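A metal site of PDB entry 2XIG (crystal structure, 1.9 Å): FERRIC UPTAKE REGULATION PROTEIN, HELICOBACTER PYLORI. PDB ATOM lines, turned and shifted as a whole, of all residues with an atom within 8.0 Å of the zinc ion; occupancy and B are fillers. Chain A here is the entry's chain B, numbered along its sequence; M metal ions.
O of Phe 111 is in hydrogen-bond range of N of Asp 98, at 2.8 Å. A ring nitrogen (NE2) of His 134 sits close to the side-chain amide oxygen (OE1) of Gln 120, at 3.4 Å.
The zinc ion is bound by OE1 of Glu 117 (2.1 Å), NE2 of His 96 (2.1 Å), NE2 of His 134 (2.1 Å) and OD1 of Asp 98 (2.2 Å). Slightly farther from the zinc ion lies the side-chain carboxylate (OD2) of Asp 98 (2.7 Å).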
ATOM      1  N   HIS A  96      17.824   8.668  -2.339  1.00  0.00           N
ATOM      2  CA  HIS A  96      18.272   7.906  -1.191  1.00  0.00           C
ATOM      3  C   HIS A  96      18.183   8.678   0.102  1.00  0.00           C
ATOM      4  O   HIS A  96      18.524   9.866   0.166  1.00  0.00           O
ATOM      5  CB  HIS A  96      19.705   7.417  -1.358  1.00  0.00           C
ATOM      6  CG  HIS A  96      20.276   6.883  -0.090  1.00  0.00           C
ATOM      7  ND1 HIS A  96      20.013   5.612   0.369  1.00  0.00           N
ATOM      8  CD2 HIS A  96      21.054   7.465   0.853  1.00  0.00           C
ATOM      9  CE1 HIS A  96      20.627   5.418   1.520  1.00  0.00           C
ATOM     10  NE2 HIS A  96      21.271   6.530   1.841  1.00  0.00           N
ATOM     11  N   HIS A  97      17.746   8.003   1.150  1.00  0.00           N
ATOM     12  CA  HIS A  97      17.776   8.582   2.477  1.00  0.00           C
ATOM     13  C   HIS A  97      17.719   7.476   3.509  1.00  0.00           C
ATOM     14  O   HIS A  97      17.326   6.354   3.206  1.00  0.00           O
ATOM     15  CB  HIS A  97      16.610   9.560   2.674  1.00  0.00           C
ATOM     16  CG  HIS A  97      15.269   8.913   2.522  1.00  0.00           C
ATOM     17  ND1 HIS A  97      14.707   8.645   1.286  1.00  0.00           N
ATOM     18  CD2 HIS A  97      14.378   8.474   3.439  1.00  0.00           C
ATOM     19  CE1 HIS A  97      13.523   8.079   1.455  1.00  0.00           C
ATOM     20  NE2 HIS A  97      13.297   7.965   2.752  1.00  0.00           N
ATOM     21  N   ASP A  98      18.129   7.823   4.725  1.00  0.00           N
ATOM     22  CA  ASP A  98      18.041   6.901   5.839  1.00  0.00           C
ATOM     23  C   ASP A  98      16.956   7.387   6.791  1.00  0.00           C
ATOM     24  O   ASP A  98      16.317   8.399   6.525  1.00  0.00           O
ATOM     25  CB  ASP A  98      19.397   6.816   6.527  1.00  0.00           C
ATOM     26  CG  ASP A  98      20.499   6.454   5.560  1.00  0.00           C
ATOM     27  OD1 ASP A  98      21.360   7.317   5.298  1.00  0.00           O
ATOM     28  OD2 ASP A  98      20.473   5.313   5.030  1.00  0.00           O
ATOM     29  N   HIS A  99      16.737   6.674   7.890  1.00  0.00           N
ATOM     30  CA  HIS A  99      15.574   6.978   8.724  1.00  0.00           C
ATOM     31  C   HIS A  99      15.864   7.090  10.188  1.00  0.00           C
ATOM     32  O   HIS A  99      16.486   6.211  10.777  1.00  0.00           O
ATOM     33  CB  HIS A  99      14.531   5.891   8.582  1.00  0.00           C
ATOM     34  CG  HIS A  99      14.092   5.662   7.171  1.00  0.00           C
ATOM     35  ND1 HIS A  99      14.704   4.737   6.364  1.00  0.00           N
ATOM     36  CD2 HIS A  99      13.125   6.245   6.429  1.00  0.00           C
ATOM     37  CE1 HIS A  99      14.127   4.757   5.169  1.00  0.00           C
ATOM     38  NE2 HIS A  99      13.164   5.664   5.198  1.00  0.00           N
ATOM     39  N   PHE A 111      16.731  11.494   6.617  1.00  0.00           N
ATOM     40  CA  PHE A 111      17.991  12.226   6.623  1.00  0.00           C
ATOM     41  C   PHE A 111      18.970  11.591   5.653  1.00  0.00           C
ATOM     42  O   PHE A 111      18.859  10.414   5.311  1.00  0.00           O
ATOM     43  CB  PHE A 111      18.597  12.294   8.041  1.00  0.00           C
ATOM     44  CG  PHE A 111      19.196  10.983   8.507  1.00  0.00           C
ATOM     45  CD1 PHE A 111      20.543  10.735   8.362  1.00  0.00           C
ATOM     46  CD2 PHE A 111      18.389  10.006   9.053  1.00  0.00           C
ATOM     47  CE1 PHE A 111      21.089   9.536   8.775  1.00  0.00           C
ATOM     48  CE2 PHE A 111      18.928   8.798   9.469  1.00  0.00           C
ATOM     49  CZ  PHE A 111      20.290   8.571   9.337  1.00  0.00           C
ATOM     50  N   ALA A 112      19.917  12.391   5.186  1.00  0.00           N
ATOM     51  CA  ALA A 112      21.014  11.895   4.370  1.00  0.00           C
ATOM     52  C   ALA A 112      22.243  12.722   4.710  1.00  0.00           C
ATOM     53  O   ALA A 112      22.424  13.825   4.193  1.00  0.00           O
ATOM     54  CB  ALA A 112      20.677  12.006   2.886  1.00  0.00           C
ATOM     55  N   ASP A 113      23.079  12.190   5.605  1.00  0.00           N
ATOM     56  CA  ASP A 113      24.230  12.936   6.093  1.00  0.00           C
ATOM     57  C   ASP A 113      25.494  12.603   5.314  1.00  0.00           C
ATOM     58  O   ASP A 113      25.944  11.452   5.321  1.00  0.00           O
ATOM     59  CB  ASP A 113      24.458  12.674   7.581  1.00  0.00           C
ATOM     60  CG  ASP A 113      25.543  13.555   8.159  1.00  0.00           C
ATOM     61  OD1 ASP A 113      25.396  14.796   8.093  1.00  0.00           O
ATOM     62  OD2 ASP A 113      26.542  13.003   8.668  1.00  0.00           O
ATOM     63  N   ILE A 116      28.332  10.668   7.264  1.00  0.00           N
ATOM     64  CA  ILE A 116      28.017   9.256   7.454  1.00  0.00           C
ATOM     65  C   ILE A 116      28.128   8.497   6.133  1.00  0.00           C
ATOM     66  O   ILE A 116      28.754   7.448   6.067  1.00  0.00           O
ATOM     67  CB  ILE A 116      26.615   9.082   8.064  1.00  0.00           C
ATOM     68  CG1 ILE A 116      26.615   9.528   9.534  1.00  0.00           C
ATOM     69  CG2 ILE A 116      26.149   7.631   7.921  1.00  0.00           C
ATOM     70  CD1 ILE A 116      25.250   9.509  10.181  1.00  0.00           C
ATOM     71  N   GLU A 117      27.515   9.038   5.078  1.00  0.00           N
ATOM     72  CA  GLU A 117      27.578   8.415   3.750  1.00  0.00           C
ATOM     73  C   GLU A 117      29.027   8.138   3.346  1.00  0.00           C
ATOM     74  O   GLU A 117      29.356   7.032   2.921  1.00  0.00           O
ATOM     75  CB  GLU A 117      26.906   9.281   2.680  1.00  0.00           C
ATOM     76  CG  GLU A 117      25.418   9.527   2.889  1.00  0.00           C
ATOM     77  CD  GLU A 117      24.583   8.255   2.837  1.00  0.00           C
ATOM     78  OE1 GLU A 117      23.592   8.195   3.596  1.00  0.00           O
ATOM     79  OE2 GLU A 117      24.905   7.323   2.064  1.00  0.00           O
ATOM     80  N   ASN A 118      29.882   9.154   3.484  1.00  0.00           N
ATOM     81  CA  ASN A 118      31.290   8.994   3.139  1.00  0.00           C
ATOM     82  C   ASN A 118      32.027   8.002   4.034  1.00  0.00           C
ATOM     83  O   ASN A 118      32.737   7.111   3.547  1.00  0.00           O
ATOM     84  CB  ASN A 118      32.008  10.339   3.116  1.00  0.00           C
ATOM     85  CG  ASN A 118      31.381  11.325   2.144  1.00  0.00           C
ATOM     86  OD1 ASN A 118      30.752  10.929   1.161  1.00  0.00           O
ATOM     87  ND2 ASN A 118      31.538  12.614   2.427  1.00  0.00           N
ATOM     88  N   GLN A 120      30.976   5.542   5.624  1.00  0.00           N
ATOM     89  CA  GLN A 120      30.553   4.162   5.372  1.00  0.00           C
ATOM     90  C   GLN A 120      31.397   3.539   4.272  1.00  0.00           C
ATOM     91  O   GLN A 120      31.782   2.370   4.346  1.00  0.00           O
ATOM     92  CB  GLN A 120      29.077   4.116   4.998  1.00  0.00           C
ATOM     93  CG  GLN A 120      28.138   4.307   6.184  1.00  0.00           C
ATOM     94  CD  GLN A 120      26.671   4.425   5.775  1.00  0.00           C
ATOM     95  OE1 GLN A 120      26.352   4.752   4.628  1.00  0.00           O
ATOM     96  NE2 GLN A 120      25.763   4.150   6.714  1.00  0.00           N
ATOM     97  N   LEU A 131      31.019  -0.904  -1.812  1.00  0.00           N
ATOM     98  CA  LEU A 131      29.738  -0.605  -1.189  1.00  0.00           C
ATOM     99  C   LEU A 131      28.617  -0.543  -2.240  1.00  0.00           C
ATOM    100  O   LEU A 131      28.638   0.302  -3.135  1.00  0.00           O
ATOM    101  CB  LEU A 131      29.795   0.696  -0.381  1.00  0.00           C
ATOM    102  CG  LEU A 131      28.517   1.060   0.382  1.00  0.00           C
ATOM    103  CD1 LEU A 131      28.130  -0.028   1.364  1.00  0.00           C
ATOM    104  CD2 LEU A 131      28.672   2.406   1.090  1.00  0.00           C
ATOM    105  N   SER A 133      24.912  -1.039  -1.255  1.00  0.00           N
ATOM    106  CA  SER A 133      23.807  -0.327  -0.642  1.00  0.00           C
ATOM    107  C   SER A 133      23.931  -0.492   0.867  1.00  0.00           C
ATOM    108  O   SER A 133      24.829  -1.168   1.362  1.00  0.00           O
ATOM    109  CB  SER A 133      22.451  -0.878  -1.120  1.00  0.00           C
ATOM    110  OG  SER A 133      22.210  -2.165  -0.587  1.00  0.00           O
ATOM    111  N   HIS A 134      23.033   0.136   1.597  1.00  0.00           N
ATOM    112  CA  HIS A 134      23.090   0.012   3.043  1.00  0.00           C
ATOM    113  C   HIS A 134      21.717   0.251   3.633  1.00  0.00           C
ATOM    114  O   HIS A 134      20.843   0.813   2.987  1.00  0.00           O
ATOM    115  CB  HIS A 134      24.114   0.979   3.628  1.00  0.00           C
ATOM    116  CG  HIS A 134      23.827   2.405   3.325  1.00  0.00           C
ATOM    117  ND1 HIS A 134      24.236   3.019   2.162  1.00  0.00           N
ATOM    118  CD2 HIS A 134      23.188   3.357   4.046  1.00  0.00           C
ATOM    119  CE1 HIS A 134      23.854   4.283   2.177  1.00  0.00           C
ATOM    120  NE2 HIS A 134      23.221   4.517   3.317  1.00  0.00           N
ATOM    121  N   ASP A 135      21.554  -0.189   4.881  1.00  0.00           N
ATOM    122  CA  ASP A 135      20.281  -0.096   5.558  1.00  0.00           C
ATOM    123  C   ASP A 135      20.657   0.467   6.900  1.00  0.00           C
ATOM    124  O   ASP A 135      21.429  -0.128   7.642  1.00  0.00           O
ATOM    125  CB  ASP A 135      19.669  -1.493   5.684  1.00  0.00           C
ATOM    126  CG  ASP A 135      18.337  -1.480   6.411  1.00  0.00           C
ATOM    127  OD1 ASP A 135      17.800  -0.382   6.681  1.00  0.00           O
ATOM    128  OD2 ASP A 135      17.833  -2.582   6.704  1.00  0.00           O
ATOM    129  N   MET A 136      20.138   1.644   7.209  1.00  0.00           N
ATOM    130  CA  MET A 136      20.597   2.363   8.372  1.00  0.00           C
ATOM    131  C   MET A 136      19.409   3.045   8.985  1.00  0.00           C
ATOM    132  O   MET A 136      18.734   3.847   8.330  1.00  0.00           O
ATOM    133  CB  MET A 136      21.636   3.376   7.929  1.00  0.00           C
ATOM    134  CG  MET A 136      22.545   3.874   9.010  1.00  0.00           C
ATOM    135  SD  MET A 136      21.855   5.322   9.807  1.00  0.00           S
ATOM    136  CE  MET A 136      23.374   6.239  10.091  1.00  0.00           C
HETATM  137 ZN    ZN M   1      22.412   6.452   3.615  1.00  0.00          ZN
